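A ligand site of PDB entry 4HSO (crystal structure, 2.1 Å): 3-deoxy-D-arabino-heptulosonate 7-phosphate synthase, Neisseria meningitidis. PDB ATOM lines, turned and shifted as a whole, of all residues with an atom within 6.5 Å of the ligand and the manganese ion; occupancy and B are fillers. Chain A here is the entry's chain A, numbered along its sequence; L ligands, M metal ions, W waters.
NH1 of Arg 167 lies within salt-bridge range of O4 of the ligand (2.9 Å).
O5 of the ligand sits at hydrogen-bond distance from N of Ala 166.
An oxygen (O2) of the ligand sits close to a ring nitrogen (NE2) of His 270 (3.1 Å).
O6 of the ligand lies within salt-bridge range of NZ of Lys 188, 2.9 Å away.
The guanidinium group (NE) of Arg 236 is in salt-bridge range of an oxygen (O6) of the ligand, at 2.8 Å.
NZ of Lys 99 is in salt-bridge range of O2 of the ligand (2.8 Å).
The guanidinium group (NH2) of Arg 94 lies within salt-bridge range of an oxygen (O2) of the ligand (2.7 Å).
N of Arg 236 is in hydrogen-bond range of OD1 of Asn 189.
The backbone carbonyl oxygen of Cys 63 is in hydrogen-bond range of the guanidinium group of Arg 94 (3.0 Å).
The backbone carbonyl oxygen (O) of Cys 63 sits at hydrogen-bond distance from the side-chain amino group (NZ) of Lys 99 (3.0 Å).
NZ of Lys 188 lies within hydrogen-bond range of SD of Met 302.
The side-chain sulfur (SG) of Cys 63 lies close to the side-chain hydroxyl (OG1) of Thr 323, at 3.0 Å.
NE of Arg 94 lies within hydrogen-bond range of O of Pro 62 (2.9 Å).
The side-chain carboxylate of Asp 267 lies within hydrogen-bond range of a ring nitrogen (ND1) of His 270, at 2.8 Å.
The side-chain carboxylate (OE1) of Glu 304 lies within hydrogen-bond range of the side-chain hydroxyl (OG) of Ser 269 (2.7 Å).
Residues that only touch the ligand: Tyr 96 (3.6 Å), Gly 165 (3.6 Å), Glu 145 (3.7 Å) and Met 302 (3.98 Å).
Hydrophobic or aromatic side chains within 4 Å of the ligand: Tyr 96, Ala 166, His 270 and Met 302.
12 residues have an atom within 4 Å of the ligand: Arg 94, Tyr 96, Lys 99, Glu 145, Gly 165, Ala 166, Arg 167, Lys 188, Arg 236, His 270, Met 302 and Glu 304.
The nearest printed residue that does not touch the ligand is Pro 100 (4.1 Å).
Four residues have an atom within 4 Å of the manganese ion: Cys 63, His 270, Glu 304 and Asp 324.
The manganese ion is bound by the side-chain carboxylate of Asp 324 (1.9 Å), the side-chain carboxylate of Glu 304 (2.1 Å), a ring nitrogen (NE2) of His 270 (2.2 Å) and the side-chain sulfur of Cys 63 (2.6 Å).
The manganese ion has four donor atoms within binding distance.
Slightly farther from the manganese ion lies O2 of the ligand (2.8 Å).
Water W4 lies within hydrogen-bond range of O1 of the ligand (2.5 Å), OH of Tyr 96 (2.9 Å), NZ of Lys 188 (3.2 Å) and SD of Met 302 (3.6 Å).
Water W1 lies within hydrogen-bond range of N of Arg 167 (2.9 Å), O5 of the ligand (3.0 Å) and N of Ala 166 (3.2 Å).
Water W3 lies within hydrogen-bond range of the side-chain carboxylate (OE1) of Glu 145 (2.6 Å) and an oxygen (O5) of the ligand (3.4 Å).
Water W2 lies within hydrogen-bond range of the side-chain carboxylate (OE1) of Glu 145 (2.6 Å), the side-chain amino group (NZ) of Lys 99 (2.8 Å) and the backbone carbonyl oxygen (O) of Glu 98 (2.9 Å).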
ATOM      1  N   PRO A  62     -14.522  -3.148  15.225  1.00  0.00           N
ATOM      2  CA  PRO A  62     -14.826  -4.160  16.231  1.00  0.00           C
ATOM      3  C   PRO A  62     -16.247  -4.108  16.762  1.00  0.00           C
ATOM      4  O   PRO A  62     -16.872  -3.068  16.753  1.00  0.00           O
ATOM      5  CB  PRO A  62     -13.833  -3.843  17.332  1.00  0.00           C
ATOM      6  CG  PRO A  62     -12.644  -3.316  16.611  1.00  0.00           C
ATOM      7  CD  PRO A  62     -13.219  -2.507  15.470  1.00  0.00           C
ATOM      8  N   CYS A  63     -16.756  -5.258  17.162  1.00  0.00           N
ATOM      9  CA  CYS A  63     -17.994  -5.311  17.846  1.00  0.00           C
ATOM     10  C   CYS A  63     -17.858  -4.344  19.057  1.00  0.00           C
ATOM     11  O   CYS A  63     -18.640  -3.438  19.241  1.00  0.00           O
ATOM     12  CB  CYS A  63     -18.295  -6.755  18.286  1.00  0.00           C
ATOM     13  SG  CYS A  63     -19.857  -6.905  19.255  1.00  0.00           S
ATOM     14  N   SER A  64     -16.810  -4.553  19.829  1.00  0.00           N
ATOM     15  CA  SER A  64     -16.546  -3.743  21.006  1.00  0.00           C
ATOM     16  C   SER A  64     -15.102  -3.416  21.113  1.00  0.00           C
ATOM     17  O   SER A  64     -14.233  -4.205  20.654  1.00  0.00           O
ATOM     18  CB  SER A  64     -16.987  -4.489  22.248  1.00  0.00           C
ATOM     19  OG  SER A  64     -16.288  -5.694  22.421  1.00  0.00           O
ATOM     20  N   ARG A  94     -15.990   1.823  13.728  1.00  0.00           N
ATOM     21  CA  ARG A  94     -16.837   1.436  14.850  1.00  0.00           C
ATOM     22  C   ARG A  94     -15.965   1.533  16.121  1.00  0.00           C
ATOM     23  O   ARG A  94     -14.980   0.782  16.223  1.00  0.00           O
ATOM     24  CB  ARG A  94     -17.285  -0.026  14.790  1.00  0.00           C
ATOM     25  CG  ARG A  94     -18.416  -0.320  13.848  1.00  0.00           C
ATOM     26  CD  ARG A  94     -18.888  -1.773  13.911  1.00  0.00           C
ATOM     27  NE  ARG A  94     -19.186  -2.285  15.250  1.00  0.00           N
ATOM     28  CZ  ARG A  94     -20.392  -2.595  15.698  1.00  0.00           C
ATOM     29  NH1 ARG A  94     -21.458  -2.370  14.962  1.00  0.00           N
ATOM     30  NH2 ARG A  94     -20.538  -3.052  16.928  1.00  0.00           N
ATOM     31  N   TYR A  96     -17.271   1.279  19.641  1.00  0.00           N
ATOM     32  CA  TYR A  96     -18.344   0.942  20.557  1.00  0.00           C
ATOM     33  C   TYR A  96     -17.802   0.606  21.952  1.00  0.00           C
ATOM     34  O   TYR A  96     -17.101  -0.397  22.122  1.00  0.00           O
ATOM     35  CB  TYR A  96     -19.149  -0.219  20.050  1.00  0.00           C
ATOM     36  CG  TYR A  96     -20.128   0.114  18.977  1.00  0.00           C
ATOM     37  CD1 TYR A  96     -19.768   0.919  17.892  1.00  0.00           C
ATOM     38  CD2 TYR A  96     -21.402  -0.413  18.986  1.00  0.00           C
ATOM     39  CE1 TYR A  96     -20.669   1.215  16.883  1.00  0.00           C
ATOM     40  CE2 TYR A  96     -22.301  -0.154  17.927  1.00  0.00           C
ATOM     41  CZ  TYR A  96     -21.917   0.687  16.904  1.00  0.00           C
ATOM     42  OH  TYR A  96     -22.827   0.985  15.834  1.00  0.00           O
ATOM     43  N   GLU A  98     -20.098   0.918  24.683  1.00  0.00           N
ATOM     44  CA  GLU A  98     -21.272   0.425  25.438  1.00  0.00           C
ATOM     45  C   GLU A  98     -22.013  -0.710  24.717  1.00  0.00           C
ATOM     46  O   GLU A  98     -22.469  -0.555  23.600  1.00  0.00           O
ATOM     47  CB  GLU A  98     -22.217   1.589  25.709  1.00  0.00           C
ATOM     48  CG  GLU A  98     -21.584   2.754  26.441  1.00  0.00           C
ATOM     49  CD  GLU A  98     -22.517   3.908  26.721  1.00  0.00           C
ATOM     50  OE1 GLU A  98     -23.461   4.161  25.963  1.00  0.00           O
ATOM     51  OE2 GLU A  98     -22.253   4.619  27.697  1.00  0.00           O
ATOM     52  N   LYS A  99     -22.116  -1.867  25.377  1.00  0.00           N
ATOM     53  CA  LYS A  99     -22.644  -3.090  24.798  1.00  0.00           C
ATOM     54  C   LYS A  99     -23.888  -3.628  25.549  1.00  0.00           C
ATOM     55  O   LYS A  99     -23.815  -3.911  26.773  1.00  0.00           O
ATOM     56  CB  LYS A  99     -21.584  -4.179  24.766  1.00  0.00           C
ATOM     57  CG  LYS A  99     -20.323  -3.778  24.057  1.00  0.00           C
ATOM     58  CD  LYS A  99     -20.566  -3.318  22.625  1.00  0.00           C
ATOM     59  CE  LYS A  99     -21.132  -4.451  21.720  1.00  0.00           C
ATOM     60  NZ  LYS A  99     -21.369  -3.933  20.354  1.00  0.00           N
ATOM     61  N   PRO A 100     -24.987  -3.865  24.823  1.00  0.00           N
ATOM     62  CA  PRO A 100     -26.195  -4.327  25.490  1.00  0.00           C
ATOM     63  C   PRO A 100     -26.225  -5.851  25.512  1.00  0.00           C
ATOM     64  O   PRO A 100     -26.142  -6.477  24.466  1.00  0.00           O
ATOM     65  CB  PRO A 100     -27.315  -3.743  24.614  1.00  0.00           C
ATOM     66  CG  PRO A 100     -26.734  -3.612  23.247  1.00  0.00           C
ATOM     67  CD  PRO A 100     -25.230  -3.440  23.437  1.00  0.00           C
ATOM     68  N   GLU A 145     -22.328   3.346  19.732  1.00  0.00           N
ATOM     69  CA  GLU A 145     -23.714   3.197  20.146  1.00  0.00           C
ATOM     70  C   GLU A 145     -23.917   3.962  21.396  1.00  0.00           C
ATOM     71  O   GLU A 145     -23.201   3.817  22.363  1.00  0.00           O
ATOM     72  CB  GLU A 145     -24.138   1.752  20.362  1.00  0.00           C
ATOM     73  CG  GLU A 145     -25.643   1.626  20.654  1.00  0.00           C
ATOM     74  CD  GLU A 145     -26.098   0.275  21.176  1.00  0.00           C
ATOM     75  OE1 GLU A 145     -25.505  -0.744  20.801  1.00  0.00           O
ATOM     76  OE2 GLU A 145     -27.156   0.210  21.866  1.00  0.00           O
ATOM     77  N   ALA A 163     -25.396   5.199  16.746  1.00  0.00           N
ATOM     78  CA  ALA A 163     -26.373   4.184  16.543  1.00  0.00           C
ATOM     79  C   ALA A 163     -27.167   4.065  17.798  1.00  0.00           C
ATOM     80  O   ALA A 163     -26.627   4.310  18.928  1.00  0.00           O
ATOM     81  CB  ALA A 163     -25.727   2.858  16.323  1.00  0.00           C
ATOM     82  N   ILE A 164     -28.457   3.816  17.612  1.00  0.00           N
ATOM     83  CA  ILE A 164     -29.338   3.439  18.787  1.00  0.00           C
ATOM     84  C   ILE A 164     -29.673   1.999  18.507  1.00  0.00           C
ATOM     85  O   ILE A 164     -30.187   1.687  17.419  1.00  0.00           O
ATOM     86  CB  ILE A 164     -30.606   4.277  18.861  1.00  0.00           C
ATOM     87  CG1 ILE A 164     -30.285   5.740  19.153  1.00  0.00           C
ATOM     88  CG2 ILE A 164     -31.587   3.719  19.920  1.00  0.00           C
ATOM     89  CD1 ILE A 164     -29.648   6.029  20.511  1.00  0.00           C
ATOM     90  N   GLY A 165     -29.321   1.122  19.401  1.00  0.00           N
ATOM     91  CA  GLY A 165     -29.427  -0.284  19.202  1.00  0.00           C
ATOM     92  C   GLY A 165     -30.846  -0.802  19.045  1.00  0.00           C
ATOM     93  O   GLY A 165     -31.800  -0.146  19.451  1.00  0.00           O
ATOM     94  N   ALA A 166     -30.956  -2.010  18.518  1.00  0.00           N
ATOM     95  CA  ALA A 166     -32.203  -2.702  18.304  1.00  0.00           C
ATOM     96  C   ALA A 166     -33.023  -2.798  19.565  1.00  0.00           C
ATOM     97  O   ALA A 166     -34.254  -2.720  19.512  1.00  0.00           O
ATOM     98  CB  ALA A 166     -31.921  -4.091  17.786  1.00  0.00           C
ATOM     99  N   ARG A 167     -32.353  -2.929  20.684  1.00  0.00           N
ATOM    100  CA  ARG A 167     -32.974  -3.113  21.942  1.00  0.00           C
ATOM    101  C   ARG A 167     -33.537  -1.850  22.555  1.00  0.00           C
ATOM    102  O   ARG A 167     -34.182  -1.910  23.522  1.00  0.00           O
ATOM    103  CB  ARG A 167     -32.074  -3.891  22.900  1.00  0.00           C
ATOM    104  CG  ARG A 167     -31.799  -5.322  22.443  1.00  0.00           C
ATOM    105  CD  ARG A 167     -30.607  -5.973  23.101  1.00  0.00           C
ATOM    106  NE  ARG A 167     -30.256  -7.233  22.452  1.00  0.00           N
ATOM    107  CZ  ARG A 167     -29.532  -7.372  21.344  1.00  0.00           C
ATOM    108  NH1 ARG A 167     -29.037  -6.344  20.707  1.00  0.00           N
ATOM    109  NH2 ARG A 167     -29.295  -8.559  20.871  1.00  0.00           N
ATOM    110  N   LYS A 188     -31.848   1.044  14.605  1.00  0.00           N
ATOM    111  CA  LYS A 188     -31.925  -0.343  14.120  1.00  0.00           C
ATOM    112  C   LYS A 188     -33.312  -0.824  14.255  1.00  0.00           C
ATOM    113  O   LYS A 188     -34.004  -0.399  15.183  1.00  0.00           O
ATOM    114  CB  LYS A 188     -30.996  -1.244  14.945  1.00  0.00           C
ATOM    115  CG  LYS A 188     -29.553  -0.884  14.699  1.00  0.00           C
ATOM    116  CD  LYS A 188     -28.567  -1.893  15.211  1.00  0.00           C
ATOM    117  CE  LYS A 188     -27.480  -2.094  14.140  1.00  0.00           C
ATOM    118  NZ  LYS A 188     -26.584  -3.194  14.533  1.00  0.00           N
ATOM    119  N   ASN A 189     -33.715  -1.728  13.345  1.00  0.00           N
ATOM    120  CA  ASN A 189     -34.929  -2.444  13.482  1.00  0.00           C
ATOM    121  C   ASN A 189     -34.876  -3.414  14.706  1.00  0.00           C
ATOM    122  O   ASN A 189     -33.795  -3.722  15.214  1.00  0.00           O
ATOM    123  CB  ASN A 189     -35.327  -3.198  12.195  1.00  0.00           C
ATOM    124  CG  ASN A 189     -34.421  -4.386  11.875  1.00  0.00           C
ATOM    125  OD1 ASN A 189     -33.672  -4.368  10.889  1.00  0.00           O
ATOM    126  ND2 ASN A 189     -34.479  -5.422  12.698  1.00  0.00           N
ATOM    127  N   THR A 191     -35.188  -6.535  17.453  1.00  0.00           N
ATOM    128  CA  THR A 191     -34.497  -7.803  17.455  1.00  0.00           C
ATOM    129  C   THR A 191     -35.288  -8.919  16.769  1.00  0.00           C
ATOM    130  O   THR A 191     -34.684  -9.886  16.343  1.00  0.00           O
ATOM    131  CB  THR A 191     -34.091  -8.258  18.865  1.00  0.00           C
ATOM    132  OG1 THR A 191     -35.211  -8.134  19.723  1.00  0.00           O
ATOM    133  CG2 THR A 191     -32.933  -7.403  19.408  1.00  0.00           C
ATOM    134  N   ARG A 236     -30.955  -4.767  10.187  1.00  0.00           N
ATOM    135  CA  ARG A 236     -30.034  -5.650  10.844  1.00  0.00           C
ATOM    136  C   ARG A 236     -30.547  -7.043  11.093  1.00  0.00           C
ATOM    137  O   ARG A 236     -29.971  -7.786  11.909  1.00  0.00           O
ATOM    138  CB  ARG A 236     -29.548  -5.006  12.189  1.00  0.00           C
ATOM    139  CG  ARG A 236     -30.624  -4.604  13.181  1.00  0.00           C
ATOM    140  CD  ARG A 236     -31.258  -5.771  13.899  1.00  0.00           C
ATOM    141  NE  ARG A 236     -30.422  -6.331  14.938  1.00  0.00           N
ATOM    142  CZ  ARG A 236     -30.661  -7.491  15.569  1.00  0.00           C
ATOM    143  NH1 ARG A 236     -29.840  -7.889  16.531  1.00  0.00           N
ATOM    144  NH2 ARG A 236     -31.685  -8.246  15.247  1.00  0.00           N
ATOM    145  N   ASP A 267     -26.835  -3.629   7.842  1.00  0.00           N
ATOM    146  CA  ASP A 267     -25.844  -4.196   8.704  1.00  0.00           C
ATOM    147  C   ASP A 267     -25.559  -5.578   8.090  1.00  0.00           C
ATOM    148  O   ASP A 267     -26.452  -6.351   7.928  1.00  0.00           O
ATOM    149  CB  ASP A 267     -26.385  -4.331  10.133  1.00  0.00           C
ATOM    150  CG  ASP A 267     -25.356  -4.870  11.138  1.00  0.00           C
ATOM    151  OD1 ASP A 267     -24.248  -5.239  10.777  1.00  0.00           O
ATOM    152  OD2 ASP A 267     -25.702  -4.949  12.359  1.00  0.00           O
ATOM    153  N   SER A 269     -23.804  -7.814   9.684  1.00  0.00           N
ATOM    154  CA  SER A 269     -23.511  -8.706  10.800  1.00  0.00           C
ATOM    155  C   SER A 269     -24.778  -9.019  11.628  1.00  0.00           C
ATOM    156  O   SER A 269     -25.887  -8.937  11.080  1.00  0.00           O
ATOM    157  CB  SER A 269     -22.394  -8.100  11.712  1.00  0.00           C
ATOM    158  OG  SER A 269     -21.825  -9.094  12.537  1.00  0.00           O
ATOM    159  N   HIS A 270     -24.612  -9.363  12.902  1.00  0.00           N
ATOM    160  CA  HIS A 270     -25.721  -9.723  13.779  1.00  0.00           C
ATOM    161  C   HIS A 270     -26.794 -10.630  13.056  1.00  0.00           C
ATOM    162  O   HIS A 270     -26.445 -11.678  12.553  1.00  0.00           O
ATOM    163  CB  HIS A 270     -26.279  -8.444  14.367  1.00  0.00           C
ATOM    164  CG  HIS A 270     -25.204  -7.622  14.994  1.00  0.00           C
ATOM    165  ND1 HIS A 270     -24.596  -6.574  14.340  1.00  0.00           N
ATOM    166  CD2 HIS A 270     -24.530  -7.766  16.165  1.00  0.00           C
ATOM    167  CE1 HIS A 270     -23.655  -6.058  15.096  1.00  0.00           C
ATOM    168  NE2 HIS A 270     -23.596  -6.770  16.204  1.00  0.00           N
ATOM    169  N   ALA A 271     -28.070 -10.292  13.095  1.00  0.00           N
ATOM    170  CA  ALA A 271     -29.142 -11.224  12.554  1.00  0.00           C
ATOM    171  C   ALA A 271     -29.153 -11.331  11.037  1.00  0.00           C
ATOM    172  O   ALA A 271     -29.713 -12.255  10.477  1.00  0.00           O
ATOM    173  CB  ALA A 271     -30.537 -10.842  13.071  1.00  0.00           C
ATOM    174  N   MET A 302     -22.823  -1.618   7.517  1.00  0.00           N
ATOM    175  CA  MET A 302     -22.173  -1.811   8.765  1.00  0.00           C
ATOM    176  C   MET A 302     -21.501  -3.158   8.772  1.00  0.00           C
ATOM    177  O   MET A 302     -22.075  -4.122   8.284  1.00  0.00           O
ATOM    178  CB  MET A 302     -23.229  -1.694   9.899  1.00  0.00           C
ATOM    179  CG  MET A 302     -22.651  -1.934  11.272  1.00  0.00           C
ATOM    180  SD  MET A 302     -23.787  -1.554  12.656  1.00  0.00           S
ATOM    181  CE  MET A 302     -24.792  -0.272  11.908  1.00  0.00           C
ATOM    182  N   GLU A 304     -18.673  -5.850  11.041  1.00  0.00           N
ATOM    183  CA  GLU A 304     -17.936  -6.173  12.276  1.00  0.00           C
ATOM    184  C   GLU A 304     -16.621  -6.826  11.880  1.00  0.00           C
ATOM    185  O   GLU A 304     -16.602  -7.937  11.322  1.00  0.00           O
ATOM    186  CB  GLU A 304     -18.786  -7.028  13.231  1.00  0.00           C
ATOM    187  CG  GLU A 304     -19.893  -6.222  13.902  1.00  0.00           C
ATOM    188  CD  GLU A 304     -20.576  -6.935  15.029  1.00  0.00           C
ATOM    189  OE1 GLU A 304     -20.923  -8.127  14.853  1.00  0.00           O
ATOM    190  OE2 GLU A 304     -20.726  -6.296  16.127  1.00  0.00           O
ATOM    191  N   THR A 323     -16.435  -9.943  22.142  1.00  0.00           N
ATOM    192  CA  THR A 323     -17.912  -9.967  22.012  1.00  0.00           C
ATOM    193  C   THR A 323     -18.323 -10.755  20.764  1.00  0.00           C
ATOM    194  O   THR A 323     -17.983 -11.907  20.677  1.00  0.00           O
ATOM    195  CB  THR A 323     -18.511  -8.560  22.186  1.00  0.00           C
ATOM    196  OG1 THR A 323     -17.836  -7.601  21.372  1.00  0.00           O
ATOM    197  CG2 THR A 323     -18.346  -8.152  23.705  1.00  0.00           C
ATOM    198  N   ASP A 324     -19.090 -10.185  19.839  1.00  0.00           N
ATOM    199  CA  ASP A 324     -19.424 -10.915  18.612  1.00  0.00           C
ATOM    200  C   ASP A 324     -18.184 -11.166  17.783  1.00  0.00           C
ATOM    201  O   ASP A 324     -17.222 -10.385  17.826  1.00  0.00           O
ATOM    202  CB  ASP A 324     -20.489 -10.191  17.756  1.00  0.00           C
ATOM    203  CG  ASP A 324     -21.739  -9.875  18.529  1.00  0.00           C
ATOM    204  OD1 ASP A 324     -22.113 -10.673  19.365  1.00  0.00           O
ATOM    205  OD2 ASP A 324     -22.290  -8.738  18.316  1.00  0.00           O
HETATM  206  C1  LIG L   1     -23.836  -3.760  17.414  1.00  0.00           C
HETATM  207  O1  LIG L   1     -23.847  -3.035  16.353  1.00  0.00           O
HETATM  208  O2  LIG L   1     -22.782  -4.260  17.910  1.00  0.00           O
HETATM  209  C2  LIG L   1     -25.106  -4.084  18.096  1.00  0.00           C
HETATM  210  C3  LIG L   1     -25.225  -4.144  19.432  1.00  0.00           C
HETATM  211  O3  LIG L   1     -26.238  -4.293  17.187  1.00  0.00           O
HETATM  212  P1  LIG L   1     -27.752  -4.824  17.475  1.00  0.00           P
HETATM  213  O4  LIG L   1     -27.645  -6.088  18.206  1.00  0.00           O
HETATM  214  O5  LIG L   1     -28.377  -3.639  18.222  1.00  0.00           O
HETATM  215  O6  LIG L   1     -28.154  -5.147  16.003  1.00  0.00           O
HETATM  216 MN    MN M   1     -21.958  -6.921  17.729  1.00  0.00          MN
HETATM  217  O   HOH W   1     -29.480  -3.405  20.987  1.00  0.00           O
HETATM  218  O   HOH W   2     -23.275  -1.997  21.201  1.00  0.00           O
HETATM  219  O   HOH W   3     -26.189  -0.980  18.258  1.00  0.00           O
HETATM  220  O   HOH W   4     -25.018  -0.868  15.983  1.00  0.00           O
